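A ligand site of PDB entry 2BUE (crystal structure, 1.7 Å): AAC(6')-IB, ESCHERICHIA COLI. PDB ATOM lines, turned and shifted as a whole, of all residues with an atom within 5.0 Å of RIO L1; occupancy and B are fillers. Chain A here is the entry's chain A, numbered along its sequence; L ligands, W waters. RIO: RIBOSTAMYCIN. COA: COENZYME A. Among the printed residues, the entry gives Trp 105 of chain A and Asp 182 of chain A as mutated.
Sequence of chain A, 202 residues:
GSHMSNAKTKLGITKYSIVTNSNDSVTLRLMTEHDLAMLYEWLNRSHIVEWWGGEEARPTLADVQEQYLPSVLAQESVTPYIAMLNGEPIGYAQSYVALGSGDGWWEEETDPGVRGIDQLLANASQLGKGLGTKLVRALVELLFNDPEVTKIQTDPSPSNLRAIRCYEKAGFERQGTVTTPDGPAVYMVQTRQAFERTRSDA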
ATOM      1  N   TRP A  51      -5.030  -4.637  11.157  1.00  0.00           N
ATOM      2  CA  TRP A  51      -6.135  -5.013  12.061  1.00  0.00           C
ATOM      3  C   TRP A  51      -7.144  -3.880  12.290  1.00  0.00           C
ATOM      4  O   TRP A  51      -8.110  -4.039  13.024  1.00  0.00           O
ATOM      5  CB  TRP A  51      -5.565  -5.453  13.412  1.00  0.00           C
ATOM      6  CG  TRP A  51      -4.666  -6.651  13.341  1.00  0.00           C
ATOM      7  CD1 TRP A  51      -3.333  -6.705  13.641  1.00  0.00           C
ATOM      8  CD2 TRP A  51      -5.033  -7.977  12.914  1.00  0.00           C
ATOM      9  NE1 TRP A  51      -2.846  -7.981  13.446  1.00  0.00           N
ATOM     10  CE2 TRP A  51      -3.868  -8.783  12.992  1.00  0.00           C
ATOM     11  CE3 TRP A  51      -6.236  -8.556  12.480  1.00  0.00           C
ATOM     12  CZ2 TRP A  51      -3.872 -10.143  12.655  1.00  0.00           C
ATOM     13  CZ3 TRP A  51      -6.241  -9.912  12.134  1.00  0.00           C
ATOM     14  CH2 TRP A  51      -5.057 -10.680  12.216  1.00  0.00           C
ATOM     15  N   TRP A  52      -6.902  -2.733  11.669  1.00  0.00           N
ATOM     16  CA  TRP A  52      -7.687  -1.556  11.950  1.00  0.00           C
ATOM     17  C   TRP A  52      -7.956  -0.800  10.688  1.00  0.00           C
ATOM     18  O   TRP A  52      -7.020  -0.402   9.988  1.00  0.00           O
ATOM     19  CB  TRP A  52      -6.948  -0.621  12.901  1.00  0.00           C
ATOM     20  CG  TRP A  52      -7.817   0.417  13.535  1.00  0.00           C
ATOM     21  CD1 TRP A  52      -8.440   1.491  12.916  1.00  0.00           C
ATOM     22  CD2 TRP A  52      -8.179   0.482  14.913  1.00  0.00           C
ATOM     23  NE1 TRP A  52      -9.171   2.211  13.845  1.00  0.00           N
ATOM     24  CE2 TRP A  52      -9.011   1.618  15.081  1.00  0.00           C
ATOM     25  CE3 TRP A  52      -7.874  -0.311  16.034  1.00  0.00           C
ATOM     26  CZ2 TRP A  52      -9.540   1.978  16.312  1.00  0.00           C
ATOM     27  CZ3 TRP A  52      -8.396   0.061  17.269  1.00  0.00           C
ATOM     28  CH2 TRP A  52      -9.225   1.192  17.402  1.00  0.00           C
ATOM     29  N   GLY A  53      -9.231  -0.588  10.409  1.00  0.00           N
ATOM     30  CA  GLY A  53      -9.627   0.196   9.272  1.00  0.00           C
ATOM     31  C   GLY A  53     -10.708  -0.517   8.501  1.00  0.00           C
ATOM     32  O   GLY A  53     -11.785   0.044   8.270  1.00  0.00           O
ATOM     33  N   GLY A  54     -10.431  -1.768   8.118  1.00  0.00           N
ATOM     34  CA  GLY A  54     -11.367  -2.539   7.273  1.00  0.00           C
ATOM     35  C   GLY A  54     -11.499  -1.852   5.932  1.00  0.00           C
ATOM     36  O   GLY A  54     -10.488  -1.604   5.256  1.00  0.00           O
ATOM     37  N   TYR A  68     -12.613  11.093  13.487  1.00  0.00           N
ATOM     38  CA  TYR A  68     -12.100  10.878  14.858  1.00  0.00           C
ATOM     39  C   TYR A  68     -12.103  12.142  15.725  1.00  0.00           C
ATOM     40  O   TYR A  68     -11.706  12.093  16.896  1.00  0.00           O
ATOM     41  CB  TYR A  68     -10.703  10.246  14.869  1.00  0.00           C
ATOM     42  CG  TYR A  68     -10.678   8.797  14.423  1.00  0.00           C
ATOM     43  CD1 TYR A  68     -10.725   7.769  15.375  1.00  0.00           C
ATOM     44  CD2 TYR A  68     -10.604   8.471  13.068  1.00  0.00           C
ATOM     45  CE1 TYR A  68     -10.678   6.450  14.985  1.00  0.00           C
ATOM     46  CE2 TYR A  68     -10.581   7.130  12.660  1.00  0.00           C
ATOM     47  CZ  TYR A  68     -10.624   6.123  13.620  1.00  0.00           C
ATOM     48  OH  TYR A  68     -10.589   4.810  13.235  1.00  0.00           O
ATOM     49  N   LEU A  73     -17.098  11.710  17.160  1.00  0.00           N
ATOM     50  CA  LEU A  73     -17.189  10.398  17.813  1.00  0.00           C
ATOM     51  C   LEU A  73     -18.313  10.423  18.877  1.00  0.00           C
ATOM     52  O   LEU A  73     -19.035   9.427  19.043  1.00  0.00           O
ATOM     53  CB  LEU A  73     -15.856  10.024  18.465  1.00  0.00           C
ATOM     54  CG  LEU A  73     -14.709   9.701  17.484  1.00  0.00           C
ATOM     55  CD1 LEU A  73     -13.418   9.488  18.301  1.00  0.00           C
ATOM     56  CD2 LEU A  73     -15.083   8.476  16.652  1.00  0.00           C
ATOM     57  N   GLU A  76     -21.741   9.226  18.032  1.00  0.00           N
ATOM     58  CA  GLU A  76     -21.872   7.771  17.952  1.00  0.00           C
ATOM     59  C   GLU A  76     -21.695   7.108  19.320  1.00  0.00           C
ATOM     60  O   GLU A  76     -21.512   5.882  19.399  1.00  0.00           O
ATOM     61  CB  GLU A  76     -20.776   7.225  17.041  1.00  0.00           C
ATOM     62  CG  GLU A  76     -21.218   6.051  16.227  1.00  0.00           C
ATOM     63  CD  GLU A  76     -21.764   6.480  14.891  1.00  0.00           C
ATOM     64  OE1 GLU A  76     -21.933   5.586  14.032  1.00  0.00           O
ATOM     65  OE2 GLU A  76     -22.003   7.695  14.681  1.00  0.00           O
ATOM     66  N   VAL A  78     -19.116   7.333  21.204  1.00  0.00           N
ATOM     67  CA  VAL A  78     -17.740   6.870  21.282  1.00  0.00           C
ATOM     68  C   VAL A  78     -16.875   7.935  21.948  1.00  0.00           C
ATOM     69  O   VAL A  78     -16.929   9.139  21.592  1.00  0.00           O
ATOM     70  CB  VAL A  78     -17.168   6.525  19.855  1.00  0.00           C
ATOM     71  CG1 VAL A  78     -15.667   6.172  19.927  1.00  0.00           C
ATOM     72  CG2 VAL A  78     -17.965   5.373  19.199  1.00  0.00           C
ATOM     73  N   TYR A  92      -3.824   4.357  21.077  1.00  0.00           N
ATOM     74  CA  TYR A  92      -5.145   4.953  20.976  1.00  0.00           C
ATOM     75  C   TYR A  92      -6.134   3.938  21.535  1.00  0.00           C
ATOM     76  O   TYR A  92      -6.003   2.747  21.293  1.00  0.00           O
ATOM     77  CB  TYR A  92      -5.493   5.255  19.506  1.00  0.00           C
ATOM     78  CG  TYR A  92      -6.953   5.592  19.303  1.00  0.00           C
ATOM     79  CD1 TYR A  92      -7.408   6.904  19.445  1.00  0.00           C
ATOM     80  CD2 TYR A  92      -7.878   4.593  18.937  1.00  0.00           C
ATOM     81  CE1 TYR A  92      -8.778   7.216  19.254  1.00  0.00           C
ATOM     82  CE2 TYR A  92      -9.254   4.890  18.751  1.00  0.00           C
ATOM     83  CZ  TYR A  92      -9.684   6.220  18.921  1.00  0.00           C
ATOM     84  OH  TYR A  92     -10.999   6.558  18.736  1.00  0.00           O
ATOM     85  N   GLN A  94     -10.632   3.522  22.563  1.00  0.00           N
ATOM     86  CA  GLN A  94     -11.955   4.150  22.586  1.00  0.00           C
ATOM     87  C   GLN A  94     -12.894   3.259  23.373  1.00  0.00           C
ATOM     88  O   GLN A  94     -12.697   2.026  23.403  1.00  0.00           O
ATOM     89  CB  GLN A  94     -12.491   4.407  21.182  1.00  0.00           C
ATOM     90  CG  GLN A  94     -12.558   3.137  20.308  1.00  0.00           C
ATOM     91  CD  GLN A  94     -13.086   3.406  18.909  1.00  0.00           C
ATOM     92  OE1 GLN A  94     -12.805   4.453  18.305  1.00  0.00           O
ATOM     93  NE2 GLN A  94     -13.816   2.436  18.371  1.00  0.00           N
ATOM     94  N   TYR A  96     -17.278   2.777  24.039  1.00  0.00           N
ATOM     95  CA  TYR A  96     -18.540   3.154  23.425  1.00  0.00           C
ATOM     96  C   TYR A  96     -19.704   2.566  24.206  1.00  0.00           C
ATOM     97  O   TYR A  96     -19.555   1.536  24.884  1.00  0.00           O
ATOM     98  CB  TYR A  96     -18.604   2.782  21.909  1.00  0.00           C
ATOM     99  CG  TYR A  96     -18.408   1.301  21.641  1.00  0.00           C
ATOM    100  CD1 TYR A  96     -19.496   0.423  21.710  1.00  0.00           C
ATOM    101  CD2 TYR A  96     -17.129   0.782  21.340  1.00  0.00           C
ATOM    102  CE1 TYR A  96     -19.344  -0.953  21.504  1.00  0.00           C
ATOM    103  CE2 TYR A  96     -16.978  -0.626  21.131  1.00  0.00           C
ATOM    104  CZ  TYR A  96     -18.079  -1.461  21.221  1.00  0.00           C
ATOM    105  OH  TYR A  96     -17.983  -2.825  21.027  1.00  0.00           O
ATOM    106  N   SER A 101     -24.775   2.515  19.476  1.00  0.00           N
ATOM    107  CA  SER A 101     -23.891   2.393  18.338  1.00  0.00           C
ATOM    108  C   SER A 101     -24.627   2.580  17.022  1.00  0.00           C
ATOM    109  O   SER A 101     -25.860   2.518  16.979  1.00  0.00           O
ATOM    110  CB  SER A 101     -23.189   1.035  18.402  1.00  0.00           C
ATOM    111  OG  SER A 101     -22.514   0.920  19.647  1.00  0.00           O
ATOM    112  N   TRP A 105     -24.899  -2.280  14.519  1.00  0.00           N
ATOM    113  CA  TRP A 105     -24.042  -2.610  15.659  1.00  0.00           C
ATOM    114  C   TRP A 105     -24.851  -2.896  16.925  1.00  0.00           C
ATOM    115  O   TRP A 105     -25.701  -2.070  17.319  1.00  0.00           O
ATOM    116  CB  TRP A 105     -23.053  -1.465  15.929  1.00  0.00           C
ATOM    117  CG  TRP A 105     -21.984  -1.346  14.913  1.00  0.00           C
ATOM    118  CD1 TRP A 105     -21.927  -0.445  13.870  1.00  0.00           C
ATOM    119  CD2 TRP A 105     -20.786  -2.110  14.853  1.00  0.00           C
ATOM    120  NE1 TRP A 105     -20.747  -0.624  13.161  1.00  0.00           N
ATOM    121  CE2 TRP A 105     -20.048  -1.668  13.719  1.00  0.00           C
ATOM    122  CE3 TRP A 105     -20.284  -3.178  15.620  1.00  0.00           C
ATOM    123  CZ2 TRP A 105     -18.806  -2.233  13.347  1.00  0.00           C
ATOM    124  CZ3 TRP A 105     -19.053  -3.741  15.261  1.00  0.00           C
ATOM    125  CH2 TRP A 105     -18.324  -3.269  14.131  1.00  0.00           C
ATOM    126  N   TRP A 106     -24.581  -4.046  17.547  1.00  0.00           N
ATOM    127  CA  TRP A 106     -25.134  -4.423  18.855  1.00  0.00           C
ATOM    128  C   TRP A 106     -26.645  -4.293  18.905  1.00  0.00           C
ATOM    129  O   TRP A 106     -27.203  -3.813  19.895  1.00  0.00           O
ATOM    130  CB  TRP A 106     -24.416  -3.650  20.010  1.00  0.00           C
ATOM    131  CG  TRP A 106     -22.950  -3.642  19.719  1.00  0.00           C
ATOM    132  CD1 TRP A 106     -22.148  -2.555  19.486  1.00  0.00           C
ATOM    133  CD2 TRP A 106     -22.120  -4.800  19.497  1.00  0.00           C
ATOM    134  NE1 TRP A 106     -20.872  -2.955  19.152  1.00  0.00           N
ATOM    135  CE2 TRP A 106     -20.822  -4.325  19.158  1.00  0.00           C
ATOM    136  CE3 TRP A 106     -22.339  -6.186  19.578  1.00  0.00           C
ATOM    137  CZ2 TRP A 106     -19.753  -5.191  18.866  1.00  0.00           C
ATOM    138  CZ3 TRP A 106     -21.269  -7.057  19.273  1.00  0.00           C
ATOM    139  CH2 TRP A 106     -19.987  -6.559  18.946  1.00  0.00           C
ATOM    140  N   ASP A 118     -12.075  -0.647  22.057  1.00  0.00           N
ATOM    141  CA  ASP A 118     -11.158  -0.987  20.938  1.00  0.00           C
ATOM    142  C   ASP A 118      -9.873  -0.249  21.237  1.00  0.00           C
ATOM    143  O   ASP A 118      -9.893   0.816  21.862  1.00  0.00           O
ATOM    144  CB  ASP A 118     -11.713  -0.495  19.609  1.00  0.00           C
ATOM    145  CG  ASP A 118     -13.102  -1.022  19.306  1.00  0.00           C
ATOM    146  OD1 ASP A 118     -13.224  -2.195  18.934  1.00  0.00           O
ATOM    147  OD2 ASP A 118     -14.051  -0.229  19.442  1.00  0.00           O
ATOM    148  N   ASP A 155     -14.701  -7.108  20.663  1.00  0.00           N
ATOM    149  CA  ASP A 155     -15.122  -7.895  19.493  1.00  0.00           C
ATOM    150  C   ASP A 155     -13.994  -8.077  18.468  1.00  0.00           C
ATOM    151  O   ASP A 155     -14.164  -7.704  17.299  1.00  0.00           O
ATOM    152  CB  ASP A 155     -16.381  -7.280  18.865  1.00  0.00           C
ATOM    153  CG  ASP A 155     -16.117  -5.918  18.195  1.00  0.00           C
ATOM    154  OD1 ASP A 155     -15.171  -5.209  18.626  1.00  0.00           O
ATOM    155  OD2 ASP A 155     -16.818  -5.602  17.209  1.00  0.00           O
ATOM    156  N   ASP A 182     -18.596  -5.348  10.644  1.00  0.00           N
ATOM    157  CA  ASP A 182     -17.213  -5.611  10.239  1.00  0.00           C
ATOM    158  C   ASP A 182     -16.941  -7.117  10.117  1.00  0.00           C
ATOM    159  O   ASP A 182     -15.781  -7.552  10.164  1.00  0.00           O
ATOM    160  CB  ASP A 182     -16.219  -4.978  11.215  1.00  0.00           C
ATOM    161  CG  ASP A 182     -16.180  -3.441  11.088  1.00  0.00           C
ATOM    162  OD1 ASP A 182     -16.696  -2.932  10.060  1.00  0.00           O
ATOM    163  OD2 ASP A 182     -15.633  -2.770  11.984  1.00  0.00           O
HETATM  164  O1  RIO L   1     -12.816   3.491  14.942  1.00  0.00           O
HETATM  165  C1  RIO L   1     -13.680   4.628  15.136  1.00  0.00           C
HETATM  166  C2  RIO L   1     -14.867   4.503  14.178  1.00  0.00           C
HETATM  167  O2  RIO L   1     -15.192   3.129  13.901  1.00  0.00           O
HETATM  168  C3  RIO L   1     -16.190   2.669  14.833  1.00  0.00           C
HETATM  169  O3  RIO L   1     -15.612   1.780  15.805  1.00  0.00           O
HETATM  170  C4  RIO L   1     -16.299   0.465  15.890  1.00  0.00           C
HETATM  171  C5  RIO L   1     -17.511   0.513  16.874  1.00  0.00           C
HETATM  172  O4  RIO L   1     -18.487   1.423  16.416  1.00  0.00           O
HETATM  173  C6  RIO L   1     -18.166  -0.861  17.127  1.00  0.00           C
HETATM  174  N1  RIO L   1     -19.179  -0.719  18.211  1.00  0.00           N
HETATM  175  C7  RIO L   1     -17.092  -1.892  17.565  1.00  0.00           C
HETATM  176  C8  RIO L   1     -15.970  -1.979  16.506  1.00  0.00           C
HETATM  177  N2  RIO L   1     -15.009  -3.048  16.928  1.00  0.00           N
HETATM  178  C9  RIO L   1     -15.257  -0.599  16.327  1.00  0.00           C
HETATM  179  O5  RIO L   1     -14.332  -0.791  15.219  1.00  0.00           O
HETATM  180  C10 RIO L   1     -13.068  -0.146  15.412  1.00  0.00           C
HETATM  181  O6  RIO L   1     -12.189  -0.969  16.129  1.00  0.00           O
HETATM  182  C11 RIO L   1     -11.725  -2.185  15.434  1.00  0.00           C
HETATM  183  C12 RIO L   1     -10.657  -2.819  16.360  1.00  0.00           C
HETATM  184  N3  RIO L   1     -11.293  -3.534  17.481  1.00  0.00           N
HETATM  185  C13 RIO L   1     -11.117  -1.845  14.048  1.00  0.00           C
HETATM  186  O7  RIO L   1     -10.833  -3.086  13.360  1.00  0.00           O
HETATM  187  C14 RIO L   1     -12.108  -0.985  13.227  1.00  0.00           C
HETATM  188  O8  RIO L   1     -11.604  -0.651  11.904  1.00  0.00           O
HETATM  189  C15 RIO L   1     -12.524   0.271  14.012  1.00  0.00           C
HETATM  190  N4  RIO L   1     -13.515   1.080  13.300  1.00  0.00           N
HETATM  191  C16 RIO L   1     -16.809   3.958  15.445  1.00  0.00           C
HETATM  192  O9  RIO L   1     -18.179   3.971  15.086  1.00  0.00           O
HETATM  193  C17 RIO L   1     -16.157   5.113  14.664  1.00  0.00           C
HETATM  194  O10 RIO L   1     -16.994   5.378  13.504  1.00  0.00           O
HETATM  195  N1A COA L   2      -0.731 -15.030  17.752  1.00  0.00           N
HETATM  196  C2A COA L   2      -1.291 -15.508  18.861  1.00  0.00           C
HETATM  197  N3A COA L   2      -0.920 -15.084  20.060  1.00  0.00           N
HETATM  198  C4A COA L   2       0.043 -14.153  20.160  1.00  0.00           C
HETATM  199  C5A COA L   2       0.652 -13.628  19.033  1.00  0.00           C
HETATM  200  C6A COA L   2       0.242 -14.093  17.798  1.00  0.00           C
HETATM  201  N6A COA L   2       0.810 -13.607  16.680  1.00  0.00           N
HETATM  202  N7A COA L   2       1.556 -12.738  19.418  1.00  0.00           N
HETATM  203  C8A COA L   2       1.535 -12.695  20.750  1.00  0.00           C
HETATM  204  N9A COA L   2       0.617 -13.553  21.197  1.00  0.00           N
HETATM  205  C1B COA L   2       0.261 -13.794  22.590  1.00  0.00           C
HETATM  206  C2B COA L   2       1.445 -13.329  23.415  1.00  0.00           C
HETATM  207  O2B COA L   2       2.295 -14.461  23.655  1.00  0.00           O
HETATM  208  C3B COA L   2       0.761 -12.799  24.672  1.00  0.00           C
HETATM  209  O3B COA L   2       0.314 -13.908  25.464  1.00  0.00           O
HETATM  210  P3B COA L   2       1.243 -14.520  26.612  1.00  0.00           P
HETATM  211  O7A COA L   2       0.267 -15.532  27.414  1.00  0.00           O
HETATM  212  O8A COA L   2       1.598 -13.318  27.624  1.00  0.00           O
HETATM  213  O9A COA L   2       2.449 -15.190  26.053  1.00  0.00           O
HETATM  214  C4B COA L   2      -0.496 -12.126  24.092  1.00  0.00           C
HETATM  215  O4B COA L   2      -0.791 -12.804  22.848  1.00  0.00           O
HETATM  216  C5B COA L   2      -0.511 -10.607  23.875  1.00  0.00           C
HETATM  217  O5B COA L   2      -0.441  -9.874  25.101  1.00  0.00           O
HETATM  218  P1A COA L   2       0.338  -8.451  25.089  1.00  0.00           P
HETATM  219  O1A COA L   2      -0.103  -7.609  26.263  1.00  0.00           O
HETATM  220  O2A COA L   2       1.795  -8.593  24.863  1.00  0.00           O
HETATM  221  O3A COA L   2      -0.313  -7.813  23.780  1.00  0.00           O
HETATM  222  P2A COA L   2       0.233  -6.449  23.071  1.00  0.00           P
HETATM  223  O4A COA L   2       0.994  -5.665  24.062  1.00  0.00           O
HETATM  224  O5A COA L   2       0.821  -6.749  21.729  1.00  0.00           O
HETATM  225  O6A COA L   2      -1.186  -5.719  22.820  1.00  0.00           O
HETATM  226  CBP COA L   2      -2.721  -5.318  20.978  1.00  0.00           C
HETATM  227  CCP COA L   2      -2.245  -6.327  22.038  1.00  0.00           C
HETATM  228  CDP COA L   2      -3.807  -6.002  20.121  1.00  0.00           C
HETATM  229  CEP COA L   2      -3.298  -4.074  21.708  1.00  0.00           C
HETATM  230  CAP COA L   2      -1.501  -4.908  20.078  1.00  0.00           C
HETATM  231  OAP COA L   2      -0.777  -6.076  19.642  1.00  0.00           O
HETATM  232  C9P COA L   2      -1.906  -4.017  18.880  1.00  0.00           C
HETATM  233  O9P COA L   2      -2.239  -2.840  19.070  1.00  0.00           O
HETATM  234  N8P COA L   2      -1.862  -4.608  17.672  1.00  0.00           N
HETATM  235  C7P COA L   2      -2.220  -3.906  16.417  1.00  0.00           C
HETATM  236  C6P COA L   2      -3.668  -3.357  16.473  1.00  0.00           C
HETATM  237  C5P COA L   2      -4.717  -4.373  16.973  1.00  0.00           C
HETATM  238  O5P COA L   2      -4.670  -5.559  16.665  1.00  0.00           O
HETATM  239  N4P COA L   2      -5.695  -3.861  17.745  1.00  0.00           N
HETATM  240  C3P COA L   2      -6.749  -4.727  18.312  1.00  0.00           C
HETATM  241  C2P COA L   2      -7.937  -4.922  17.378  1.00  0.00           C
HETATM  242  S1P COA L   2      -9.307  -5.873  18.182  1.00  0.00           S
HETATM  243  O   HOH W   1     -16.456   6.780  11.281  1.00  0.00           O
HETATM  244  O   HOH W   2     -15.872  -0.194  12.299  1.00  0.00           O
HETATM  245  O   HOH W   3     -12.089  -5.016  19.705  1.00  0.00           O
HETATM  246  O   HOH W   4      -9.491  -6.238  13.278  1.00  0.00           O
HETATM  247  O   HOH W   5     -12.260  -5.448  13.612  1.00  0.00           O
HETATM  248  O   HOH W   6     -14.653  -4.083  14.188  1.00  0.00           O
HETATM  249  O   HOH W   7     -13.447  -1.904  10.187  1.00  0.00           O
HETATM  250  O   HOH W   8     -11.991  -4.299  10.686  1.00  0.00           O
HETATM  251  O   HOH W   9     -12.634   2.129  10.785  1.00  0.00           O
HETATM  252  O   HOH W  10     -12.901  -5.408  16.197  1.00  0.00           O
HETATM  253  O   HOH W  11     -16.700   8.579  13.153  1.00  0.00           O
HETATM  254  O   HOH W  12     -13.945   5.811  11.224  1.00  0.00           O
HETATM  255  O   HOH W  13      -9.342  -3.433  19.649  1.00  0.00           O
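The side-chain carboxylate (OD1) of Asp 155 is in salt-bridge range of a nitrogen (N2) of RIO L1, 2.8 Å away.
N3 of RIO L1 is in salt-bridge range of OD1 of Asp 118, at 2.8 Å.
An oxygen (O8) of RIO L1 lies within hydrogen-bond range of the backbone NH (N) of Gly 53 (2.8 Å).
O of Trp 51 sits at hydrogen-bond distance from O7 of RIO L1 (2.9 Å).
The indole nitrogen (NE1) of Trp 106 lies close to a nitrogen (N1) of RIO L1 (3.0 Å).
O1 of RIO L1 is in hydrogen-bond range of OH of Tyr 68 (3.1 Å).
The side-chain amide nitrogen (NE2) of Gln 94 sits at hydrogen-bond distance from an oxygen (O3) of RIO L1, at 3.2 Å.
A sulfur (S1P) of COA L2 lies close to a nitrogen (N3) of RIO L1 (3.1 Å).
OD2 of Asp 118 lies within hydrogen-bond range of NE2 of Gln 94.
The indole nitrogen of Trp 106 lies close to the side-chain hydroxyl of Tyr 96 (3.4 Å).
NE1 of Trp 52 is in hydrogen-bond range of OH of Tyr 68 (3.0 Å).
The side-chain hydroxyl of Tyr 92 is in hydrogen-bond range of the side-chain amide oxygen of Gln 94, 2.8 Å away.
CE3 of Trp 52 touches C12 of RIO L1, 3.8 Å away.
CG of Glu 76 touches O9 of RIO L1, at 3.9 Å.
Tyr 96 touches RIO L1.
Ser 101 touches RIO L1 (OG to N1, 3.98 Å).
Trp 105 touches RIO L1 (CE3 to C6, 3.5 Å).
Hydrophobic or aromatic side chains within 4 Å of RIO L1: Trp 52, Tyr 68, Tyr 96, Trp 105 and Trp 106.
Of the 17 residues printed, 12 come within 4 Å of RIO L1.
Along chain A the residues within 4 Å of RIO L1 span positions 51 to 155.
The nearest printed residue that does not touch RIO L1 is Asp 182 (4.01 Å).
Water W10 bridges N3 of RIO L1 (2.8 Å) and O of Asp 155 (2.8 Å).
Water W3 lies within hydrogen-bond range of a nitrogen (N3) of RIO L1 (2.8 Å), the side-chain carboxylate (OD1) of Asp 118 (3.1 Å), the side-chain carboxylate (OD1) of Asp 155 (3.3 Å) and a sulfur (S1P) of COA L2 (3.3 Å).
Water W7 lies within hydrogen-bond range of an oxygen (O8) of RIO L1 (2.8 Å), the side-chain carboxylate of Asp 182 (3.0 Å) and the backbone carbonyl oxygen of Gly 53 (3.2 Å).
Water W2 lies within hydrogen-bond range of the side-chain carboxylate of Asp 182 (2.6 Å) and a nitrogen (N4) of RIO L1 (2.9 Å).
Water W13 lies within hydrogen-bond range of S1P of COA L2 (2.8 Å) and N3 of RIO L1 (2.9 Å).
Water W4 bridges the backbone carbonyl oxygen (O) of Trp 51 and an oxygen (O7) of RIO L1.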
